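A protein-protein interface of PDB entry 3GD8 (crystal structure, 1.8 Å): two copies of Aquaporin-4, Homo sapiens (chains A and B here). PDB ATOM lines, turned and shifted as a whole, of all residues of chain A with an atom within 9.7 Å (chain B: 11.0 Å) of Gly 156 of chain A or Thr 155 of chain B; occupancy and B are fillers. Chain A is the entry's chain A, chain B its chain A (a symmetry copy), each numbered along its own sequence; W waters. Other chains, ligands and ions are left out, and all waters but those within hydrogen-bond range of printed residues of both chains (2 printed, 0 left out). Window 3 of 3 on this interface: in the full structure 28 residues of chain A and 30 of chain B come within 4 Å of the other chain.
Gly 156 of chain A touches Thr 155 of chain B, but with the chains exchanged Thr 155 of chain A does not touch Gly 156 of chain B (6.2 Å).
Gly 156 of chain A touches its own counterpart, Gly 156 of chain B.
Ser 157 of chain A touches Gly 156 of chain B, but with the chains exchanged Gly 156 of chain A does not touch Ser 157 of chain B (5.8 Å).
Ile 158 of chain A touches Thr 155 of chain B, but with the chains exchanged Thr 155 of chain A does not touch Ile 158 of chain B (11.6 Å).
Positions printed for both chains: 146, 147, 152, 153, 154, 155, 156, 157, 158, 159, 160, 161 and 162.
O of Ala 145 of chain B is in hydrogen-bond range of NH1 of Arg 151 of chain B (3.0 Å).
The side-chain hydroxyl (OG) of Ser 157 of chain A lies within hydrogen-bond range of the backbone NH (N) of Leu 160 of chain A, at 2.9 Å.
The guanidinium group (NE) of Arg 151 of chain B lies within salt-bridge range of the side-chain carboxylate (OD1) of Asp 153 of chain B (2.9 Å).
OG of Ser 157 of chain A sits at hydrogen-bond distance from N of Ala 159 of chain A.
The backbone carbonyl oxygen (O) of Thr 142 of chain B sits at hydrogen-bond distance from the side-chain hydroxyl (OG) of Ser 146 of chain B, at 2.8 Å.
Gly 156 of chain A touches just these residues of chain B: Thr 155 and Gly 156.
No residue of chain B comes within 4 Å of Thr 155 of chain A.
Of chain B, only Thr 155 (2.9 Å) comes within 4 Å of Ile 158 of chain A.
Of chain A, only Gly 156 and Ser 157 come within 4 Å of Gly 156 of chain B.
Of the printed residues of chain B, Gln 55 of chain A touches Ala 145, Ser 146, Arg 151 and Ala 161.
Of the printed residues of chain B, Leu 160 of chain A touches Phe 164.
Of the printed residues of chain A, Asp 153 of chain B touches His 59 (3.4 Å).
Of the printed residues of chain A, Phe 164 of chain B touches Leu 160 (3.8 Å).
Printed residues of chain A within 4 Å of Ala 161 of chain B: Gln 55.
Cys 147 of chain A touches none of the printed residues of chain B.
Ile 158 of chain B touches none of the printed residues of chain A.
The nearest residue of chain B that does not touch Gly 156 of chain A is Ser 157 of chain B (5.8 Å).
The nearest printed residue of chain A that does not touch Ala 145 of chain B is His 59 of chain A (4.3 Å).
The side-chain amide nitrogen of Gln 55 of chain A is in hydrogen-bond range of the side-chain hydroxyl of Ser 146 of chain B (2.8 Å).
N of Ile 158 of chain A is in hydrogen-bond range of OG1 of Thr 155 of chain B, 2.9 Å away.
O of Gln 55 of chain A is in hydrogen-bond range of NH1 of Arg 151 of chain B (2.9 Å).
A ring nitrogen (ND1) of His 59 of chain A sits close to the guanidinium group (NH2) of Arg 151 of chain B, 3.4 Å away.
Of the 17 printed residues of chain A, 6 touch a printed residue of chain B.
Printed residues of chain A that touch a printed residue of chain B: Gln 55, His 59, Gly 156, Ser 157, Ile 158 and Leu 160.
Printed residues of chain B that touch a printed residue of chain A: Ala 145, Ser 146, Arg 151, Asp 153, Thr 155, Gly 156, Ala 161 and Phe 164.
Along chain B the printed residues that touch a printed residue of chain A span positions 145 to 164.
Among the printed residues, pairs that only touch across the chains: Gly 156 of chain A with Thr 155 of chain B (3.3 Å), Gln 55 of chain A with Ala 161 of chain B (3.4 Å), His 59 of chain A with Asp 153 of chain B (3.4 Å), Ser 157 of chain A with Thr 155 of chain B (3.5 Å), Ser 157 of chain A with Gly 156 of chain B (3.6 Å), Gly 156 of chain A with Gly 156 of chain B (3.7 Å), Leu 160 of chain A with Phe 164 of chain B (3.8 Å) and Gln 55 of chain A with Ala 145 of chain B (3.8 Å).
Water W2 lies within hydrogen-bond range of the side-chain amide oxygen of Gln 55 of chain A (2.7 Å) and the backbone carbonyl oxygen of Thr 155 of chain B (2.7 Å).
Water W1 lies within hydrogen-bond range of the backbone carbonyl oxygen (O) of Thr 155 of chain B, the side-chain amide nitrogen (NE2) of Gln 55 of chain A and the backbone carbonyl oxygen (O) of Ser 157 of chain B.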
ATOM      1  N   ALA A  51       1.651  20.465  12.677  1.00  0.00           N
ATOM      2  CA  ALA A  51       1.719  19.433  11.646  1.00  0.00           C
ATOM      3  C   ALA A  51       0.609  18.402  11.836  1.00  0.00           C
ATOM      4  O   ALA A  51      -0.038  17.974  10.879  1.00  0.00           O
ATOM      5  CB  ALA A  51       3.100  18.742  11.636  1.00  0.00           C
ATOM      6  N   VAL A  54      -2.936  19.978  11.121  1.00  0.00           N
ATOM      7  CA  VAL A  54      -3.117  20.132   9.672  1.00  0.00           C
ATOM      8  C   VAL A  54      -3.399  18.766   9.033  1.00  0.00           C
ATOM      9  O   VAL A  54      -4.267  18.638   8.152  1.00  0.00           O
ATOM     10  CB  VAL A  54      -1.901  20.831   9.013  1.00  0.00           C
ATOM     11  CG1 VAL A  54      -1.992  20.769   7.478  1.00  0.00           C
ATOM     12  CG2 VAL A  54      -1.802  22.279   9.493  1.00  0.00           C
ATOM     13  N   GLN A  55      -2.690  17.741   9.492  1.00  0.00           N
ATOM     14  CA  GLN A  55      -2.950  16.360   9.056  1.00  0.00           C
ATOM     15  C   GLN A  55      -4.398  15.953   9.363  1.00  0.00           C
ATOM     16  O   GLN A  55      -5.072  15.353   8.525  1.00  0.00           O
ATOM     17  CB  GLN A  55      -1.989  15.385   9.735  1.00  0.00           C
ATOM     18  CG  GLN A  55      -2.097  13.929   9.263  1.00  0.00           C
ATOM     19  CD  GLN A  55      -1.267  13.629   8.024  1.00  0.00           C
ATOM     20  OE1 GLN A  55      -0.657  14.523   7.435  1.00  0.00           O
ATOM     21  NE2 GLN A  55      -1.220  12.356   7.639  1.00  0.00           N
ATOM     22  N   HIS A  59      -8.286  18.739   5.301  1.00  0.00           N
ATOM     23  CA  HIS A  59      -9.320  18.396   4.325  1.00  0.00           C
ATOM     24  C   HIS A  59     -10.743  18.738   4.771  1.00  0.00           C
ATOM     25  O   HIS A  59     -11.678  18.637   3.979  1.00  0.00           O
ATOM     26  CB  HIS A  59      -9.249  16.906   3.988  1.00  0.00           C
ATOM     27  CG  HIS A  59      -9.493  16.002   5.158  1.00  0.00           C
ATOM     28  ND1 HIS A  59      -8.827  16.130   6.363  1.00  0.00           N
ATOM     29  CD2 HIS A  59     -10.315  14.936   5.293  1.00  0.00           C
ATOM     30  CE1 HIS A  59      -9.240  15.182   7.188  1.00  0.00           C
ATOM     31  NE2 HIS A  59     -10.133  14.438   6.558  1.00  0.00           N
ATOM     32  N   SER A 146       3.415  25.590  -0.287  1.00  0.00           N
ATOM     33  CA  SER A 146       3.150  24.161  -0.126  1.00  0.00           C
ATOM     34  C   SER A 146       1.825  23.737  -0.733  1.00  0.00           C
ATOM     35  O   SER A 146       1.709  22.622  -1.253  1.00  0.00           O
ATOM     36  CB  SER A 146       3.195  23.757   1.357  1.00  0.00           C
ATOM     37  OG  SER A 146       4.497  23.938   1.888  1.00  0.00           O
ATOM     38  N   CYS A 147       0.842  24.635  -0.691  1.00  0.00           N
ATOM     39  CA  CYS A 147      -0.519  24.335  -1.140  1.00  0.00           C
ATOM     40  C   CYS A 147      -0.832  24.805  -2.565  1.00  0.00           C
ATOM     41  O   CYS A 147      -1.962  24.671  -3.028  1.00  0.00           O
ATOM     42  CB  CYS A 147      -1.521  24.954  -0.166  1.00  0.00           C
ATOM     43  SG  CYS A 147      -1.351  24.313   1.509  1.00  0.00           S
ATOM     44  N   THR A 152       3.954  21.210  -9.592  1.00  0.00           N
ATOM     45  CA  THR A 152       4.033  19.780  -9.855  1.00  0.00           C
ATOM     46  C   THR A 152       5.174  19.148  -9.058  1.00  0.00           C
ATOM     47  O   THR A 152       5.370  17.930  -9.100  1.00  0.00           O
ATOM     48  CB  THR A 152       4.263  19.513 -11.356  1.00  0.00           C
ATOM     49  OG1 THR A 152       5.427  20.228 -11.799  1.00  0.00           O
ATOM     50  CG2 THR A 152       3.055  19.959 -12.168  1.00  0.00           C
ATOM     51  N   ASP A 153       5.899  19.976  -8.307  1.00  0.00           N
ATOM     52  CA  ASP A 153       7.164  19.571  -7.710  1.00  0.00           C
ATOM     53  C   ASP A 153       7.134  19.475  -6.190  1.00  0.00           C
ATOM     54  O   ASP A 153       8.167  19.201  -5.597  1.00  0.00           O
ATOM     55  CB  ASP A 153       8.272  20.549  -8.118  1.00  0.00           C
ATOM     56  CG  ASP A 153       8.082  21.932  -7.513  1.00  0.00           C
ATOM     57  OD1 ASP A 153       6.946  22.438  -7.553  1.00  0.00           O
ATOM     58  OD2 ASP A 153       9.066  22.510  -6.997  1.00  0.00           O
ATOM     59  N   VAL A 154       5.985  19.714  -5.551  1.00  0.00           N
ATOM     60  CA  VAL A 154       5.911  19.579  -4.087  1.00  0.00           C
ATOM     61  C   VAL A 154       6.044  18.104  -3.713  1.00  0.00           C
ATOM     62  O   VAL A 154       5.346  17.252  -4.254  1.00  0.00           O
ATOM     63  CB  VAL A 154       4.609  20.175  -3.491  1.00  0.00           C
ATOM     64  CG1 VAL A 154       4.564  19.953  -1.970  1.00  0.00           C
ATOM     65  CG2 VAL A 154       4.518  21.668  -3.793  1.00  0.00           C
ATOM     66  N   THR A 155       6.962  17.804  -2.793  1.00  0.00           N
ATOM     67  CA  THR A 155       7.201  16.422  -2.379  1.00  0.00           C
ATOM     68  C   THR A 155       7.035  16.255  -0.862  1.00  0.00           C
ATOM     69  O   THR A 155       7.275  17.184  -0.076  1.00  0.00           O
ATOM     70  CB  THR A 155       8.614  15.946  -2.841  1.00  0.00           C
ATOM     71  OG1 THR A 155       9.620  16.863  -2.365  1.00  0.00           O
ATOM     72  CG2 THR A 155       8.683  15.860  -4.362  1.00  0.00           C
ATOM     73  N   GLY A 156       6.616  15.063  -0.447  1.00  0.00           N
ATOM     74  CA  GLY A 156       6.502  14.757   0.975  1.00  0.00           C
ATOM     75  C   GLY A 156       5.313  15.455   1.615  1.00  0.00           C
ATOM     76  O   GLY A 156       4.416  15.939   0.923  1.00  0.00           O
ATOM     77  N   SER A 157       5.309  15.489   2.940  1.00  0.00           N
ATOM     78  CA  SER A 157       4.154  15.969   3.704  1.00  0.00           C
ATOM     79  C   SER A 157       4.045  17.485   3.713  1.00  0.00           C
ATOM     80  O   SER A 157       4.960  18.181   4.155  1.00  0.00           O
ATOM     81  CB  SER A 157       4.214  15.451   5.134  1.00  0.00           C
ATOM     82  OG  SER A 157       3.250  16.097   5.953  1.00  0.00           O
ATOM     83  N   ILE A 158       2.912  17.999   3.237  1.00  0.00           N
ATOM     84  CA  ILE A 158       2.632  19.426   3.348  1.00  0.00           C
ATOM     85  C   ILE A 158       2.476  19.834   4.823  1.00  0.00           C
ATOM     86  O   ILE A 158       2.980  20.880   5.255  1.00  0.00           O
ATOM     87  CB  ILE A 158       1.376  19.799   2.557  1.00  0.00           C
ATOM     88  CG1 ILE A 158       1.697  19.749   1.050  1.00  0.00           C
ATOM     89  CG2 ILE A 158       0.842  21.181   3.006  1.00  0.00           C
ATOM     90  CD1 ILE A 158       0.470  19.678   0.134  1.00  0.00           C
ATOM     91  N   ALA A 159       1.770  19.005   5.582  1.00  0.00           N
ATOM     92  CA  ALA A 159       1.573  19.260   7.013  1.00  0.00           C
ATOM     93  C   ALA A 159       2.919  19.399   7.750  1.00  0.00           C
ATOM     94  O   ALA A 159       3.108  20.307   8.588  1.00  0.00           O
ATOM     95  CB  ALA A 159       0.723  18.138   7.634  1.00  0.00           C
ATOM     96  N   LEU A 160       3.853  18.506   7.454  1.00  0.00           N
ATOM     97  CA  LEU A 160       5.141  18.529   8.137  1.00  0.00           C
ATOM     98  C   LEU A 160       5.947  19.762   7.727  1.00  0.00           C
ATOM     99  O   LEU A 160       6.614  20.387   8.566  1.00  0.00           O
ATOM    100  CB  LEU A 160       5.903  17.238   7.870  1.00  0.00           C
ATOM    101  CG  LEU A 160       7.061  16.853   8.766  1.00  0.00           C
ATOM    102  CD1 LEU A 160       6.706  16.972  10.280  1.00  0.00           C
ATOM    103  CD2 LEU A 160       7.492  15.420   8.382  1.00  0.00           C
ATOM    104  N   ALA A 161       5.880  20.141   6.451  1.00  0.00           N
ATOM    105  CA  ALA A 161       6.537  21.380   5.996  1.00  0.00           C
ATOM    106  C   ALA A 161       6.065  22.601   6.789  1.00  0.00           C
ATOM    107  O   ALA A 161       6.873  23.433   7.243  1.00  0.00           O
ATOM    108  CB  ALA A 161       6.319  21.597   4.485  1.00  0.00           C
ATOM    109  N   ILE A 162       4.759  22.698   6.982  1.00  0.00           N
ATOM    110  CA  ILE A 162       4.176  23.799   7.724  1.00  0.00           C
ATOM    111  C   ILE A 162       4.592  23.724   9.199  1.00  0.00           C
ATOM    112  O   ILE A 162       5.006  24.724   9.789  1.00  0.00           O
ATOM    113  CB  ILE A 162       2.659  23.818   7.569  1.00  0.00           C
ATOM    114  CG1 ILE A 162       2.282  24.108   6.109  1.00  0.00           C
ATOM    115  CG2 ILE A 162       2.016  24.859   8.487  1.00  0.00           C
ATOM    116  CD1 ILE A 162       0.833  23.811   5.775  1.00  0.00           C
ATOM    117  N   THR B 142      -5.756  11.438  14.377  1.00  0.00           N
ATOM    118  CA  THR B 142      -4.665  11.447  13.389  1.00  0.00           C
ATOM    119  C   THR B 142      -4.619  10.141  12.585  1.00  0.00           C
ATOM    120  O   THR B 142      -4.453  10.155  11.360  1.00  0.00           O
ATOM    121  CB  THR B 142      -3.289  11.714  14.062  1.00  0.00           C
ATOM    122  OG1 THR B 142      -3.339  12.976  14.726  1.00  0.00           O
ATOM    123  CG2 THR B 142      -2.147  11.728  13.037  1.00  0.00           C
ATOM    124  N   ALA B 145      -7.758  10.074  10.245  1.00  0.00           N
ATOM    125  CA  ALA B 145      -7.580  11.070   9.178  1.00  0.00           C
ATOM    126  C   ALA B 145      -6.509  10.649   8.172  1.00  0.00           C
ATOM    127  O   ALA B 145      -6.657  10.861   6.963  1.00  0.00           O
ATOM    128  CB  ALA B 145      -7.226  12.431   9.777  1.00  0.00           C
ATOM    129  N   SER B 146      -5.415  10.082   8.676  1.00  0.00           N
ATOM    130  CA  SER B 146      -4.284   9.698   7.832  1.00  0.00           C
ATOM    131  C   SER B 146      -4.593   8.508   6.941  1.00  0.00           C
ATOM    132  O   SER B 146      -4.100   8.434   5.810  1.00  0.00           O
ATOM    133  CB  SER B 146      -3.039   9.398   8.683  1.00  0.00           C
ATOM    134  OG  SER B 146      -2.598  10.566   9.357  1.00  0.00           O
ATOM    135  N   CYS B 147      -5.429   7.599   7.438  1.00  0.00           N
ATOM    136  CA  CYS B 147      -5.739   6.349   6.742  1.00  0.00           C
ATOM    137  C   CYS B 147      -7.048   6.379   5.945  1.00  0.00           C
ATOM    138  O   CYS B 147      -7.450   5.367   5.374  1.00  0.00           O
ATOM    139  CB  CYS B 147      -5.784   5.204   7.754  1.00  0.00           C
ATOM    140  SG  CYS B 147      -4.216   4.970   8.609  1.00  0.00           S
ATOM    141  N   ASP B 148      -7.703   7.534   5.900  1.00  0.00           N
ATOM    142  CA  ASP B 148      -9.002   7.673   5.236  1.00  0.00           C
ATOM    143  C   ASP B 148      -8.862   7.552   3.710  1.00  0.00           C
ATOM    144  O   ASP B 148      -8.308   8.443   3.064  1.00  0.00           O
ATOM    145  CB  ASP B 148      -9.608   9.026   5.616  1.00  0.00           C
ATOM    146  CG  ASP B 148     -10.974   9.255   5.018  1.00  0.00           C
ATOM    147  OD1 ASP B 148     -11.552  10.319   5.296  1.00  0.00           O
ATOM    148  OD2 ASP B 148     -11.473   8.383   4.278  1.00  0.00           O
ATOM    149  N   ARG B 151      -9.774  10.294   1.107  1.00  0.00           N
ATOM    150  CA  ARG B 151      -8.888  11.434   0.910  1.00  0.00           C
ATOM    151  C   ARG B 151      -7.986  11.249  -0.295  1.00  0.00           C
ATOM    152  O   ARG B 151      -7.433  10.170  -0.505  1.00  0.00           O
ATOM    153  CB  ARG B 151      -8.019  11.664   2.140  1.00  0.00           C
ATOM    154  CG  ARG B 151      -8.804  12.066   3.359  1.00  0.00           C
ATOM    155  CD  ARG B 151      -7.871  12.418   4.497  1.00  0.00           C
ATOM    156  NE  ARG B 151      -7.193  13.694   4.283  1.00  0.00           N
ATOM    157  CZ  ARG B 151      -6.420  14.294   5.187  1.00  0.00           C
ATOM    158  NH1 ARG B 151      -6.217  13.739   6.375  1.00  0.00           N
ATOM    159  NH2 ARG B 151      -5.852  15.462   4.908  1.00  0.00           N
ATOM    160  N   THR B 152      -7.849  12.316  -1.079  1.00  0.00           N
ATOM    161  CA  THR B 152      -6.918  12.357  -2.198  1.00  0.00           C
ATOM    162  C   THR B 152      -5.727  13.258  -1.876  1.00  0.00           C
ATOM    163  O   THR B 152      -4.796  13.380  -2.678  1.00  0.00           O
ATOM    164  CB  THR B 152      -7.617  12.885  -3.468  1.00  0.00           C
ATOM    165  OG1 THR B 152      -8.217  14.160  -3.192  1.00  0.00           O
ATOM    166  CG2 THR B 152      -8.690  11.910  -3.930  1.00  0.00           C
ATOM    167  N   ASP B 153      -5.745  13.857  -0.686  1.00  0.00           N
ATOM    168  CA  ASP B 153      -4.826  14.937  -0.350  1.00  0.00           C
ATOM    169  C   ASP B 153      -3.805  14.576   0.720  1.00  0.00           C
ATOM    170  O   ASP B 153      -3.032  15.438   1.111  1.00  0.00           O
ATOM    171  CB  ASP B 153      -5.615  16.166   0.116  1.00  0.00           C
ATOM    172  CG  ASP B 153      -6.314  15.941   1.448  1.00  0.00           C
ATOM    173  OD1 ASP B 153      -6.935  14.874   1.611  1.00  0.00           O
ATOM    174  OD2 ASP B 153      -6.243  16.827   2.331  1.00  0.00           O
ATOM    175  N   VAL B 154      -3.801  13.335   1.216  1.00  0.00           N
ATOM    176  CA  VAL B 154      -2.793  12.941   2.214  1.00  0.00           C
ATOM    177  C   VAL B 154      -1.418  12.896   1.548  1.00  0.00           C
ATOM    178  O   VAL B 154      -1.246  12.277   0.503  1.00  0.00           O
ATOM    179  CB  VAL B 154      -3.113  11.583   2.891  1.00  0.00           C
ATOM    180  CG1 VAL B 154      -1.998  11.200   3.879  1.00  0.00           C
ATOM    181  CG2 VAL B 154      -4.447  11.655   3.628  1.00  0.00           C
ATOM    182  N   THR B 155      -0.442  13.575   2.152  1.00  0.00           N
ATOM    183  CA  THR B 155       0.906  13.631   1.589  1.00  0.00           C
ATOM    184  C   THR B 155       1.954  13.134   2.596  1.00  0.00           C
ATOM    185  O   THR B 155       1.791  13.259   3.819  1.00  0.00           O
ATOM    186  CB  THR B 155       1.240  15.076   1.105  1.00  0.00           C
ATOM    187  OG1 THR B 155       1.035  16.014   2.180  1.00  0.00           O
ATOM    188  CG2 THR B 155       0.363  15.463  -0.081  1.00  0.00           C
ATOM    189  N   GLY B 156       3.036  12.560   2.078  1.00  0.00           N
ATOM    190  CA  GLY B 156       4.139  12.126   2.928  1.00  0.00           C
ATOM    191  C   GLY B 156       3.791  10.875   3.719  1.00  0.00           C
ATOM    192  O   GLY B 156       2.822  10.179   3.408  1.00  0.00           O
ATOM    193  N   SER B 157       4.596  10.589   4.732  1.00  0.00           N
ATOM    194  CA  SER B 157       4.497   9.331   5.477  1.00  0.00           C
ATOM    195  C   SER B 157       3.337   9.320   6.459  1.00  0.00           C
ATOM    196  O   SER B 157       3.261  10.162   7.355  1.00  0.00           O
ATOM    197  CB  SER B 157       5.797   9.051   6.217  1.00  0.00           C
ATOM    198  OG  SER B 157       5.643   7.977   7.134  1.00  0.00           O
ATOM    199  N   ILE B 158       2.438   8.351   6.301  1.00  0.00           N
ATOM    200  CA  ILE B 158       1.377   8.146   7.280  1.00  0.00           C
ATOM    201  C   ILE B 158       1.966   7.704   8.632  1.00  0.00           C
ATOM    202  O   ILE B 158       1.542   8.170   9.698  1.00  0.00           O
ATOM    203  CB  ILE B 158       0.363   7.114   6.780  1.00  0.00           C
ATOM    204  CG1 ILE B 158      -0.486   7.746   5.658  1.00  0.00           C
ATOM    205  CG2 ILE B 158      -0.499   6.587   7.953  1.00  0.00           C
ATOM    206  CD1 ILE B 158      -1.237   6.741   4.779  1.00  0.00           C
ATOM    207  N   ALA B 159       2.936   6.801   8.574  1.00  0.00           N
ATOM    208  CA  ALA B 159       3.605   6.320   9.787  1.00  0.00           C
ATOM    209  C   ALA B 159       4.216   7.483  10.592  1.00  0.00           C
ATOM    210  O   ALA B 159       4.091   7.546  11.834  1.00  0.00           O
ATOM    211  CB  ALA B 159       4.684   5.286   9.417  1.00  0.00           C
ATOM    212  N   LEU B 160       4.880   8.399   9.901  1.00  0.00           N
ATOM    213  CA  LEU B 160       5.532   9.510  10.584  1.00  0.00           C
ATOM    214  C   LEU B 160       4.495  10.462  11.179  1.00  0.00           C
ATOM    215  O   LEU B 160       4.674  10.974  12.295  1.00  0.00           O
ATOM    216  CB  LEU B 160       6.482  10.227   9.634  1.00  0.00           C
ATOM    217  CG  LEU B 160       7.554  11.140  10.193  1.00  0.00           C
ATOM    218  CD1 LEU B 160       8.347  10.478  11.361  1.00  0.00           C
ATOM    219  CD2 LEU B 160       8.475  11.550   9.024  1.00  0.00           C
ATOM    220  N   ALA B 161       3.394  10.695  10.462  1.00  0.00           N
ATOM    221  CA  ALA B 161       2.296  11.512  11.010  1.00  0.00           C
ATOM    222  C   ALA B 161       1.784  10.961  12.342  1.00  0.00           C
ATOM    223  O   ALA B 161       1.591  11.704  13.322  1.00  0.00           O
ATOM    224  CB  ALA B 161       1.143  11.636   9.995  1.00  0.00           C
ATOM    225  N   ILE B 162       1.586   9.652  12.392  1.00  0.00           N
ATOM    226  CA  ILE B 162       1.111   8.996  13.594  1.00  0.00           C
ATOM    227  C   ILE B 162       2.172   9.081  14.699  1.00  0.00           C
ATOM    228  O   ILE B 162       1.865   9.423  15.843  1.00  0.00           O
ATOM    229  CB  ILE B 162       0.715   7.552  13.307  1.00  0.00           C
ATOM    230  CG1 ILE B 162      -0.491   7.515  12.358  1.00  0.00           C
ATOM    231  CG2 ILE B 162       0.386   6.796  14.595  1.00  0.00           C
ATOM    232  CD1 ILE B 162      -0.748   6.154  11.739  1.00  0.00           C
ATOM    233  N   PHE B 164       4.521  11.315  15.098  1.00  0.00           N
ATOM    234  CA  PHE B 164       4.618  12.668  15.643  1.00  0.00           C
ATOM    235  C   PHE B 164       3.425  13.040  16.533  1.00  0.00           C
ATOM    236  O   PHE B 164       3.581  13.828  17.468  1.00  0.00           O
ATOM    237  CB  PHE B 164       4.889  13.712  14.555  1.00  0.00           C
ATOM    238  CG  PHE B 164       6.301  13.651  13.984  1.00  0.00           C
ATOM    239  CD1 PHE B 164       7.403  13.420  14.796  1.00  0.00           C
ATOM    240  CD2 PHE B 164       6.515  13.860  12.634  1.00  0.00           C
ATOM    241  CE1 PHE B 164       8.706  13.387  14.264  1.00  0.00           C
ATOM    242  CE2 PHE B 164       7.813  13.840  12.101  1.00  0.00           C
ATOM    243  CZ  PHE B 164       8.893  13.593  12.915  1.00  0.00           C
HETATM  244  O   HOH W   1       1.190  12.006   6.121  1.00  0.00           O
HETATM  245  O   HOH W   2      -0.207  14.818   4.836  1.00  0.00           O
